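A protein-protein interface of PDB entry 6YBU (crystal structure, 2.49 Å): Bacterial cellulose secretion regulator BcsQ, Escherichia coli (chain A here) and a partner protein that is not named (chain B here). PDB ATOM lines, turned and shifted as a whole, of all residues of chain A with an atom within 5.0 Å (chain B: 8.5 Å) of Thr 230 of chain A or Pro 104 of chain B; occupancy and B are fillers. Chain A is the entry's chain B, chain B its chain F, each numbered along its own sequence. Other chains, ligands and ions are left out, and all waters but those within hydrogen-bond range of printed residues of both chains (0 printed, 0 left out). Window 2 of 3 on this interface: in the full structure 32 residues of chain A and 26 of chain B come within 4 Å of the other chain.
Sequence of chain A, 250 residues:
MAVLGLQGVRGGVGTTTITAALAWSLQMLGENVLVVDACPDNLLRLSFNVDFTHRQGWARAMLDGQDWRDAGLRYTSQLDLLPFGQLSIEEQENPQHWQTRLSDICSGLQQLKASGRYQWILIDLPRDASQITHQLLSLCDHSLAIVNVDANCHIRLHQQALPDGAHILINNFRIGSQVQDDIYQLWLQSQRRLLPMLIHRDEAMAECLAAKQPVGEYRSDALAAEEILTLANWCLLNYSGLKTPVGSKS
The backbone carbonyl oxygen (O) of Gln 62 of chain B lies close to the side-chain amide oxygen (OD1) of Asn 233 of chain A. ND2 of Asn 233 of chain A is in hydrogen-bond range of OG1 of Thr 65 of chain B (2.9 Å). The guanidinium group (NH1) of Arg 68 of chain B sits at hydrogen-bond distance from the side-chain hydroxyl (OG1) of Thr 230 of chain A (2.9 Å). The backbone carbonyl oxygen (O) of Glu 226 of chain A lies within hydrogen-bond range of the guanidinium group (NH2) of Arg 68 of chain B (3.2 Å).
The side-chain amide nitrogen (ND2) of Asn 233 of chain A lies within hydrogen-bond range of the backbone carbonyl oxygen (O) of Leu 229 of chain A. The backbone NH (N) of Arg 68 of chain B is in hydrogen-bond range of the backbone carbonyl oxygen (O) of Ile 102 of chain B. O of Glu 226 of chain A sits at hydrogen-bond distance from OG1 of Thr 230 of chain A (3.0 Å). The guanidinium group of Arg 68 of chain B is in hydrogen-bond range of the backbone carbonyl oxygen of Thr 65 of chain B (3.1 Å). The side-chain hydroxyl of Thr 65 of chain B lies within hydrogen-bond range of the backbone carbonyl oxygen of Gln 62 of chain B, at 2.5 Å.
CE of Met 197 of chain A touches CD2 of Leu 105 of chain B, 3.7 Å away. Thr 65 of chain B touches Leu 229 of chain A (CB to CD2, 3.9 Å). Leu 229 of chain A touches Arg 68 of chain B. Thr 230 of chain A touches Pro 104 of chain B. CG2 of Thr 230 of chain A touches CG of Leu 105 of chain B (3.99 Å). Ile 58 of chain B touches Asn 233 of chain A (CD1 to OD1, 3.9 Å). ND2 of Asn 233 of chain A touches CD2 of Leu 66 of chain B (3.4 Å).
Of the printed residues of chain B, Thr 230 of chain A touches Arg 68, Pro 104 and Leu 105. Pro 104 of chain B touches one residue of chain A. Printed residues of chain A within 4 Å of Leu 66 of chain B: Asn 233 (3.4 Å). Of the printed residues of chain A, Arg 68 of chain B touches Glu 226, Leu 229 and Thr 230. Of the printed residues of chain B, Met 197 of chain A touches Leu 105. Of the printed residues of chain A, Ile 58 of chain B touches Asn 233 (3.9 Å). Ala 232 of chain A touches none of the printed residues of chain B. The nearest printed residue of chain B that does not touch Thr 230 of chain A is Leu 66 of chain B (4.001 Å).
Printed residues of chain A that touch a printed residue of chain B: Met 197, Glu 226, Leu 229, Thr 230 and Asn 233. Hydrophobic or aromatic side chains of chain A that line the printed part of chain B: Met 197 and Leu 229. Of the 21 printed residues of chain B, 7 touch a printed residue of chain A. Hydrophobic or aromatic side chains of chain B that line the printed part of chain A: Ile 58, Leu 66, Pro 104 and Leu 105. Among the printed residues, 11 pairs touch across the chains. Among the printed residues, no Asp or Glu carboxylate lies within 4 Å of a Lys or Arg side-chain nitrogen of the other chain.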
ATOM      1  N   MET A 197      10.858 -28.565  27.032  1.00  0.00           N
ATOM      2  CA  MET A 197      12.269 -28.802  27.292  1.00  0.00           C
ATOM      3  C   MET A 197      12.458 -29.296  28.719  1.00  0.00           C
ATOM      4  O   MET A 197      11.635 -29.043  29.604  1.00  0.00           O
ATOM      5  CB  MET A 197      13.103 -27.536  27.052  1.00  0.00           C
ATOM      6  CG  MET A 197      13.081 -26.517  28.186  1.00  0.00           C
ATOM      7  SD  MET A 197      11.497 -25.678  28.375  1.00  0.00           S
ATOM      8  CE  MET A 197      11.286 -24.979  26.741  1.00  0.00           C
ATOM      9  N   GLU A 226      22.705 -24.639  28.386  1.00  0.00           N
ATOM     10  CA  GLU A 226      21.972 -24.390  27.151  1.00  0.00           C
ATOM     11  C   GLU A 226      20.499 -24.747  27.289  1.00  0.00           C
ATOM     12  O   GLU A 226      19.649 -24.130  26.638  1.00  0.00           O
ATOM     13  CB  GLU A 226      22.604 -25.168  25.999  1.00  0.00           C
ATOM     14  CG  GLU A 226      24.072 -24.850  25.780  1.00  0.00           C
ATOM     15  CD  GLU A 226      24.648 -25.550  24.565  1.00  0.00           C
ATOM     16  OE1 GLU A 226      23.861 -25.974  23.690  1.00  0.00           O
ATOM     17  OE2 GLU A 226      25.889 -25.680  24.485  1.00  0.00           O
ATOM     18  N   GLU A 227      20.177 -25.733  28.126  1.00  0.00           N
ATOM     19  CA  GLU A 227      18.777 -26.065  28.367  1.00  0.00           C
ATOM     20  C   GLU A 227      18.087 -24.966  29.167  1.00  0.00           C
ATOM     21  O   GLU A 227      16.967 -24.557  28.839  1.00  0.00           O
ATOM     22  CB  GLU A 227      18.680 -27.415  29.079  1.00  0.00           C
ATOM     23  CG  GLU A 227      19.071 -28.594  28.197  1.00  0.00           C
ATOM     24  CD  GLU A 227      19.359 -29.858  28.985  1.00  0.00           C
ATOM     25  OE1 GLU A 227      19.757 -29.749  30.165  1.00  0.00           O
ATOM     26  OE2 GLU A 227      19.189 -30.961  28.422  1.00  0.00           O
ATOM     27  N   ILE A 228      18.749 -24.470  30.217  1.00  0.00           N
ATOM     28  CA  ILE A 228      18.214 -23.341  30.977  1.00  0.00           C
ATOM     29  C   ILE A 228      18.039 -22.128  30.073  1.00  0.00           C
ATOM     30  O   ILE A 228      17.057 -21.383  30.189  1.00  0.00           O
ATOM     31  CB  ILE A 228      19.128 -23.022  32.175  1.00  0.00           C
ATOM     32  CG1 ILE A 228      19.160 -24.187  33.166  1.00  0.00           C
ATOM     33  CG2 ILE A 228      18.666 -21.754  32.880  1.00  0.00           C
ATOM     34  CD1 ILE A 228      17.931 -24.276  34.031  1.00  0.00           C
ATOM     35  N   LEU A 229      18.989 -21.908  29.157  1.00  0.00           N
ATOM     36  CA  LEU A 229      18.882 -20.785  28.233  1.00  0.00           C
ATOM     37  C   LEU A 229      17.670 -20.937  27.322  1.00  0.00           C
ATOM     38  O   LEU A 229      16.971 -19.957  27.034  1.00  0.00           O
ATOM     39  CB  LEU A 229      20.166 -20.658  27.412  1.00  0.00           C
ATOM     40  CG  LEU A 229      20.248 -19.471  26.452  1.00  0.00           C
ATOM     41  CD1 LEU A 229      20.026 -18.166  27.200  1.00  0.00           C
ATOM     42  CD2 LEU A 229      21.587 -19.457  25.730  1.00  0.00           C
ATOM     43  N   THR A 230      17.403 -22.161  26.859  1.00  0.00           N
ATOM     44  CA  THR A 230      16.176 -22.415  26.113  1.00  0.00           C
ATOM     45  C   THR A 230      14.950 -22.102  26.962  1.00  0.00           C
ATOM     46  O   THR A 230      13.974 -21.525  26.469  1.00  0.00           O
ATOM     47  CB  THR A 230      16.137 -23.869  25.638  1.00  0.00           C
ATOM     48  OG1 THR A 230      17.289 -24.144  24.832  1.00  0.00           O
ATOM     49  CG2 THR A 230      14.880 -24.138  24.823  1.00  0.00           C
ATOM     50  N   LEU A 231      14.989 -22.469  28.246  1.00  0.00           N
ATOM     51  CA  LEU A 231      13.875 -22.171  29.141  1.00  0.00           C
ATOM     52  C   LEU A 231      13.683 -20.668  29.303  1.00  0.00           C
ATOM     53  O   LEU A 231      12.546 -20.184  29.378  1.00  0.00           O
ATOM     54  CB  LEU A 231      14.107 -22.831  30.501  1.00  0.00           C
ATOM     55  CG  LEU A 231      13.096 -22.489  31.598  1.00  0.00           C
ATOM     56  CD1 LEU A 231      11.733 -23.094  31.285  1.00  0.00           C
ATOM     57  CD2 LEU A 231      13.594 -22.947  32.960  1.00  0.00           C
ATOM     58  N   ALA A 232      14.782 -19.913  29.364  1.00  0.00           N
ATOM     59  CA  ALA A 232      14.674 -18.463  29.484  1.00  0.00           C
ATOM     60  C   ALA A 232      14.006 -17.857  28.257  1.00  0.00           C
ATOM     61  O   ALA A 232      13.154 -16.968  28.381  1.00  0.00           O
ATOM     62  CB  ALA A 232      16.054 -17.848  29.704  1.00  0.00           C
ATOM     63  N   ASN A 233      14.377 -18.326  27.063  1.00  0.00           N
ATOM     64  CA  ASN A 233      13.731 -17.836  25.850  1.00  0.00           C
ATOM     65  C   ASN A 233      12.264 -18.239  25.809  1.00  0.00           C
ATOM     66  O   ASN A 233      11.411 -17.463  25.360  1.00  0.00           O
ATOM     67  CB  ASN A 233      14.463 -18.352  24.611  1.00  0.00           C
ATOM     68  CG  ASN A 233      15.762 -17.613  24.353  1.00  0.00           C
ATOM     69  OD1 ASN A 233      15.760 -16.449  23.947  1.00  0.00           O
ATOM     70  ND2 ASN A 233      16.882 -18.291  24.578  1.00  0.00           N
ATOM     71  N   TRP A 234      11.950 -19.456  26.265  1.00  0.00           N
ATOM     72  CA  TRP A 234      10.556 -19.875  26.348  1.00  0.00           C
ATOM     73  C   TRP A 234       9.769 -18.965  27.283  1.00  0.00           C
ATOM     74  O   TRP A 234       8.601 -18.651  27.020  1.00  0.00           O
ATOM     75  CB  TRP A 234      10.473 -21.330  26.815  1.00  0.00           C
ATOM     76  CG  TRP A 234       9.082 -21.897  26.797  1.00  0.00           C
ATOM     77  CD1 TRP A 234       8.510 -22.638  25.803  1.00  0.00           C
ATOM     78  CD2 TRP A 234       8.090 -21.772  27.824  1.00  0.00           C
ATOM     79  NE1 TRP A 234       7.224 -22.981  26.147  1.00  0.00           N
ATOM     80  CE2 TRP A 234       6.941 -22.459  27.382  1.00  0.00           C
ATOM     81  CE3 TRP A 234       8.061 -21.145  29.074  1.00  0.00           C
ATOM     82  CZ2 TRP A 234       5.778 -22.536  28.144  1.00  0.00           C
ATOM     83  CZ3 TRP A 234       6.905 -21.222  29.829  1.00  0.00           C
ATOM     84  CH2 TRP A 234       5.779 -21.914  29.362  1.00  0.00           C
ATOM     85  N   ILE B  58      10.225 -11.070  21.033  1.00  0.00           N
ATOM     86  CA  ILE B  58      11.616 -11.494  21.173  1.00  0.00           C
ATOM     87  C   ILE B  58      12.471 -10.755  20.151  1.00  0.00           C
ATOM     88  O   ILE B  58      12.093 -10.625  18.982  1.00  0.00           O
ATOM     89  CB  ILE B  58      11.748 -13.028  21.032  1.00  0.00           C
ATOM     90  CG1 ILE B  58      13.182 -13.479  21.307  1.00  0.00           C
ATOM     91  CG2 ILE B  58      11.280 -13.503  19.662  1.00  0.00           C
ATOM     92  CD1 ILE B  58      13.348 -14.986  21.314  1.00  0.00           C
ATOM     93  N   GLN B  62      18.267 -12.117  20.966  1.00  0.00           N
ATOM     94  CA  GLN B  62      17.749 -13.129  21.881  1.00  0.00           C
ATOM     95  C   GLN B  62      17.422 -14.417  21.138  1.00  0.00           C
ATOM     96  O   GLN B  62      17.787 -15.511  21.581  1.00  0.00           O
ATOM     97  CB  GLN B  62      16.512 -12.596  22.606  1.00  0.00           C
ATOM     98  CG  GLN B  62      16.795 -11.429  23.536  1.00  0.00           C
ATOM     99  CD  GLN B  62      15.534 -10.848  24.151  1.00  0.00           C
ATOM    100  OE1 GLN B  62      14.481 -10.809  23.516  1.00  0.00           O
ATOM    101  NE2 GLN B  62      15.639 -10.397  25.397  1.00  0.00           N
ATOM    102  N   ALA B  63      16.734 -14.307  19.998  1.00  0.00           N
ATOM    103  CA  ALA B  63      16.414 -15.499  19.220  1.00  0.00           C
ATOM    104  C   ALA B  63      17.668 -16.155  18.668  1.00  0.00           C
ATOM    105  O   ALA B  63      17.672 -17.361  18.399  1.00  0.00           O
ATOM    106  CB  ALA B  63      15.451 -15.154  18.086  1.00  0.00           C
ATOM    107  N   LEU B  64      18.744 -15.380  18.499  1.00  0.00           N
ATOM    108  CA  LEU B  64      20.001 -15.945  18.025  1.00  0.00           C
ATOM    109  C   LEU B  64      20.541 -16.994  18.988  1.00  0.00           C
ATOM    110  O   LEU B  64      21.175 -17.964  18.556  1.00  0.00           O
ATOM    111  CB  LEU B  64      21.025 -14.829  17.813  1.00  0.00           C
ATOM    112  CG  LEU B  64      22.421 -15.269  17.360  1.00  0.00           C
ATOM    113  CD1 LEU B  64      22.336 -16.101  16.090  1.00  0.00           C
ATOM    114  CD2 LEU B  64      23.340 -14.074  17.158  1.00  0.00           C
ATOM    115  N   THR B  65      20.280 -16.835  20.288  1.00  0.00           N
ATOM    116  CA  THR B  65      20.750 -17.807  21.269  1.00  0.00           C
ATOM    117  C   THR B  65      20.140 -19.187  21.057  1.00  0.00           C
ATOM    118  O   THR B  65      20.726 -20.184  21.492  1.00  0.00           O
ATOM    119  CB  THR B  65      20.443 -17.320  22.687  1.00  0.00           C
ATOM    120  OG1 THR B  65      19.024 -17.221  22.864  1.00  0.00           O
ATOM    121  CG2 THR B  65      21.072 -15.957  22.927  1.00  0.00           C
ATOM    122  N   LEU B  66      18.983 -19.268  20.401  1.00  0.00           N
ATOM    123  CA  LEU B  66      18.336 -20.541  20.122  1.00  0.00           C
ATOM    124  C   LEU B  66      18.825 -21.191  18.834  1.00  0.00           C
ATOM    125  O   LEU B  66      18.455 -22.337  18.557  1.00  0.00           O
ATOM    126  CB  LEU B  66      16.815 -20.358  20.049  1.00  0.00           C
ATOM    127  CG  LEU B  66      16.119 -19.834  21.309  1.00  0.00           C
ATOM    128  CD1 LEU B  66      14.684 -19.432  21.006  1.00  0.00           C
ATOM    129  CD2 LEU B  66      16.161 -20.873  22.421  1.00  0.00           C
ATOM    130  N   CYS B  67      19.645 -20.500  18.045  1.00  0.00           N
ATOM    131  CA  CYS B  67      20.123 -21.024  16.766  1.00  0.00           C
ATOM    132  C   CYS B  67      21.416 -21.789  17.019  1.00  0.00           C
ATOM    133  O   CYS B  67      22.478 -21.189  17.207  1.00  0.00           O
ATOM    134  CB  CYS B  67      20.322 -19.891  15.766  1.00  0.00           C
ATOM    135  SG  CYS B  67      20.703 -20.433  14.086  1.00  0.00           S
ATOM    136  N   ARG B  68      21.334 -23.121  17.020  1.00  0.00           N
ATOM    137  CA  ARG B  68      22.454 -23.993  17.382  1.00  0.00           C
ATOM    138  C   ARG B  68      22.687 -25.029  16.290  1.00  0.00           C
ATOM    139  O   ARG B  68      22.299 -26.197  16.430  1.00  0.00           O
ATOM    140  CB  ARG B  68      22.200 -24.668  18.730  1.00  0.00           C
ATOM    141  CG  ARG B  68      22.016 -23.681  19.866  1.00  0.00           C
ATOM    142  CD  ARG B  68      21.310 -24.304  21.056  1.00  0.00           C
ATOM    143  NE  ARG B  68      20.874 -23.278  21.998  1.00  0.00           N
ATOM    144  CZ  ARG B  68      20.145 -23.516  23.081  1.00  0.00           C
ATOM    145  NH1 ARG B  68      19.762 -24.753  23.369  1.00  0.00           N
ATOM    146  NH2 ARG B  68      19.799 -22.512  23.877  1.00  0.00           N
ATOM    147  N   PRO B  69      23.328 -24.642  15.190  1.00  0.00           N
ATOM    148  CA  PRO B  69      23.627 -25.617  14.139  1.00  0.00           C
ATOM    149  C   PRO B  69      24.731 -26.563  14.575  1.00  0.00           C
ATOM    150  O   PRO B  69      25.565 -26.246  15.425  1.00  0.00           O
ATOM    151  CB  PRO B  69      24.084 -24.753  12.959  1.00  0.00           C
ATOM    152  CG  PRO B  69      23.716 -23.350  13.329  1.00  0.00           C
ATOM    153  CD  PRO B  69      23.764 -23.290  14.818  1.00  0.00           C
ATOM    154  N   LEU B  99      15.753 -27.178  10.125  1.00  0.00           N
ATOM    155  CA  LEU B  99      15.419 -26.141  11.096  1.00  0.00           C
ATOM    156  C   LEU B  99      15.082 -26.743  12.453  1.00  0.00           C
ATOM    157  O   LEU B  99      15.486 -26.210  13.494  1.00  0.00           O
ATOM    158  CB  LEU B  99      14.255 -25.290  10.584  1.00  0.00           C
ATOM    159  CG  LEU B  99      14.542 -24.367   9.398  1.00  0.00           C
ATOM    160  CD1 LEU B  99      13.332 -23.509   9.072  1.00  0.00           C
ATOM    161  CD2 LEU B  99      15.755 -23.495   9.695  1.00  0.00           C
ATOM    162  N   ASN B 100      14.346 -27.858  12.464  1.00  0.00           N
ATOM    163  CA  ASN B 100      14.004 -28.501  13.728  1.00  0.00           C
ATOM    164  C   ASN B 100      15.237 -29.049  14.436  1.00  0.00           C
ATOM    165  O   ASN B 100      15.256 -29.125  15.669  1.00  0.00           O
ATOM    166  CB  ASN B 100      12.986 -29.618  13.494  1.00  0.00           C
ATOM    167  CG  ASN B 100      11.632 -29.090  13.062  1.00  0.00           C
ATOM    168  OD1 ASN B 100      11.342 -27.901  13.206  1.00  0.00           O
ATOM    169  ND2 ASN B 100      10.793 -29.974  12.533  1.00  0.00           N
ATOM    170  N   HIS B 101      16.272 -29.428  13.684  1.00  0.00           N
ATOM    171  CA  HIS B 101      17.513 -29.873  14.311  1.00  0.00           C
ATOM    172  C   HIS B 101      18.274 -28.714  14.940  1.00  0.00           C
ATOM    173  O   HIS B 101      18.989 -28.906  15.930  1.00  0.00           O
ATOM    174  CB  HIS B 101      18.401 -30.583  13.287  1.00  0.00           C
ATOM    175  CG  HIS B 101      17.933 -31.959  12.925  1.00  0.00           C
ATOM    176  ND1 HIS B 101      18.128 -32.503  11.674  1.00  0.00           N
ATOM    177  CD2 HIS B 101      17.291 -32.904  13.651  1.00  0.00           C
ATOM    178  CE1 HIS B 101      17.619 -33.723  11.643  1.00  0.00           C
ATOM    179  NE2 HIS B 101      17.107 -33.990  12.830  1.00  0.00           N
ATOM    180  N   ILE B 102      18.132 -27.512  14.386  1.00  0.00           N
ATOM    181  CA  ILE B 102      18.942 -26.373  14.805  1.00  0.00           C
ATOM    182  C   ILE B 102      18.303 -25.622  15.968  1.00  0.00           C
ATOM    183  O   ILE B 102      19.002 -25.168  16.877  1.00  0.00           O
ATOM    184  CB  ILE B 102      19.189 -25.453  13.594  1.00  0.00           C
ATOM    185  CG1 ILE B 102      20.016 -26.191  12.540  1.00  0.00           C
ATOM    186  CG2 ILE B 102      19.882 -24.168  14.017  1.00  0.00           C
ATOM    187  CD1 ILE B 102      20.079 -25.489  11.204  1.00  0.00           C
ATOM    188  N   PHE B 103      16.976 -25.491  15.969  1.00  0.00           N
ATOM    189  CA  PHE B 103      16.354 -24.756  17.065  1.00  0.00           C
ATOM    190  C   PHE B 103      15.700 -25.713  18.056  1.00  0.00           C
ATOM    191  O   PHE B 103      15.098 -26.713  17.650  1.00  0.00           O
ATOM    192  CB  PHE B 103      15.303 -23.778  16.534  1.00  0.00           C
ATOM    193  CG  PHE B 103      15.879 -22.640  15.734  1.00  0.00           C
ATOM    194  CD1 PHE B 103      16.157 -22.791  14.384  1.00  0.00           C
ATOM    195  CD2 PHE B 103      16.137 -21.417  16.333  1.00  0.00           C
ATOM    196  CE1 PHE B 103      16.684 -21.744  13.650  1.00  0.00           C
ATOM    197  CE2 PHE B 103      16.664 -20.370  15.605  1.00  0.00           C
ATOM    198  CZ  PHE B 103      16.938 -20.532  14.263  1.00  0.00           C
ATOM    199  N   PRO B 104      15.801 -25.435  19.360  1.00  0.00           N
ATOM    200  CA  PRO B 104      15.209 -26.338  20.358  1.00  0.00           C
ATOM    201  C   PRO B 104      13.715 -26.149  20.559  1.00  0.00           C
ATOM    202  O   PRO B 104      13.105 -26.934  21.298  1.00  0.00           O
ATOM    203  CB  PRO B 104      15.980 -25.984  21.635  1.00  0.00           C
ATOM    204  CG  PRO B 104      16.292 -24.536  21.467  1.00  0.00           C
ATOM    205  CD  PRO B 104      16.513 -24.310  19.990  1.00  0.00           C
ATOM    206  N   LEU B 105      13.114 -25.146  19.938  1.00  0.00           N
ATOM    207  CA  LEU B 105      11.689 -24.871  20.008  1.00  0.00           C
ATOM    208  C   LEU B 105      11.142 -24.774  18.594  1.00  0.00           C
ATOM    209  O   LEU B 105      11.901 -24.554  17.644  1.00  0.00           O
ATOM    210  CB  LEU B 105      11.418 -23.567  20.775  1.00  0.00           C
ATOM    211  CG  LEU B 105      11.911 -23.518  22.224  1.00  0.00           C
ATOM    212  CD1 LEU B 105      11.686 -22.139  22.827  1.00  0.00           C
ATOM    213  CD2 LEU B 105      11.227 -24.589  23.063  1.00  0.00           C
ATOM    214  N   PRO B 106       9.833 -24.959  18.413  1.00  0.00           N
ATOM    215  CA  PRO B 106       9.253 -24.818  17.070  1.00  0.00           C
ATOM    216  C   PRO B 106       9.514 -23.431  16.496  1.00  0.00           C
ATOM    217  O   PRO B 106       9.284 -22.413  17.155  1.00  0.00           O
ATOM    218  CB  PRO B 106       7.759 -25.068  17.302  1.00  0.00           C
ATOM    219  CG  PRO B 106       7.710 -25.919  18.530  1.00  0.00           C
ATOM    220  CD  PRO B 106       8.845 -25.448  19.392  1.00  0.00           C
ATOM    221  N   THR B 107      10.007 -23.403  15.254  1.00  0.00           N
ATOM    222  CA  THR B 107      10.369 -22.140  14.618  1.00  0.00           C
ATOM    223  C   THR B 107       9.165 -21.219  14.463  1.00  0.00           C
ATOM    224  O   THR B 107       9.315 -19.992  14.494  1.00  0.00           O
ATOM    225  CB  THR B 107      11.015 -22.397  13.253  1.00  0.00           C
ATOM    226  OG1 THR B 107      10.128 -23.176  12.438  1.00  0.00           O
ATOM    227  CG2 THR B 107      12.336 -23.140  13.411  1.00  0.00           C
ATOM    228  N   ASP B 109       6.957 -20.697  16.653  1.00  0.00           N
ATOM    229  CA  ASP B 109       6.797 -19.967  17.907  1.00  0.00           C
ATOM    230  C   ASP B 109       7.848 -18.881  18.088  1.00  0.00           C
ATOM    231  O   ASP B 109       7.603 -17.914  18.819  1.00  0.00           O
ATOM    232  CB  ASP B 109       6.855 -20.930  19.100  1.00  0.00           C
ATOM    233  CG  ASP B 109       5.813 -22.029  19.015  1.00  0.00           C
ATOM    234  OD1 ASP B 109       4.829 -21.847  18.270  1.00  0.00           O
ATOM    235  OD2 ASP B 109       5.980 -23.073  19.688  1.00  0.00           O
ATOM    236  N   ILE B 110       9.003 -19.015  17.441  1.00  0.00           N
ATOM    237  CA  ILE B 110      10.078 -18.041  17.585  1.00  0.00           C
ATOM    238  C   ILE B 110       9.973 -16.934  16.544  1.00  0.00           C
ATOM    239  O   ILE B 110      10.218 -15.764  16.849  1.00  0.00           O
ATOM    240  CB  ILE B 110      11.445 -18.752  17.501  1.00  0.00           C
ATOM    241  CG1 ILE B 110      11.486 -19.968  18.431  1.00  0.00           C
ATOM    242  CG2 ILE B 110      12.568 -17.782  17.838  1.00  0.00           C
ATOM    243  CD1 ILE B 110      12.717 -20.838  18.253  1.00  0.00           C
ATOM    244  N   PHE B 111       9.609 -17.275  15.310  1.00  0.00           N
ATOM    245  CA  PHE B 111       9.675 -16.349  14.188  1.00  0.00           C
ATOM    246  C   PHE B 111       8.300 -16.183  13.560  1.00  0.00           C
ATOM    247  O   PHE B 111       7.603 -17.171  13.310  1.00  0.00           O
ATOM    248  CB  PHE B 111      10.686 -16.838  13.150  1.00  0.00           C
ATOM    249  CG  PHE B 111      12.036 -17.150  13.726  1.00  0.00           C
ATOM    250  CD1 PHE B 111      12.934 -16.133  14.010  1.00  0.00           C
ATOM    251  CD2 PHE B 111      12.404 -18.458  13.995  1.00  0.00           C
ATOM    252  CE1 PHE B 111      14.175 -16.414  14.547  1.00  0.00           C
ATOM    253  CE2 PHE B 111      13.646 -18.745  14.530  1.00  0.00           C
ATOM    254  CZ  PHE B 111      14.532 -17.721  14.807  1.00  0.00           C
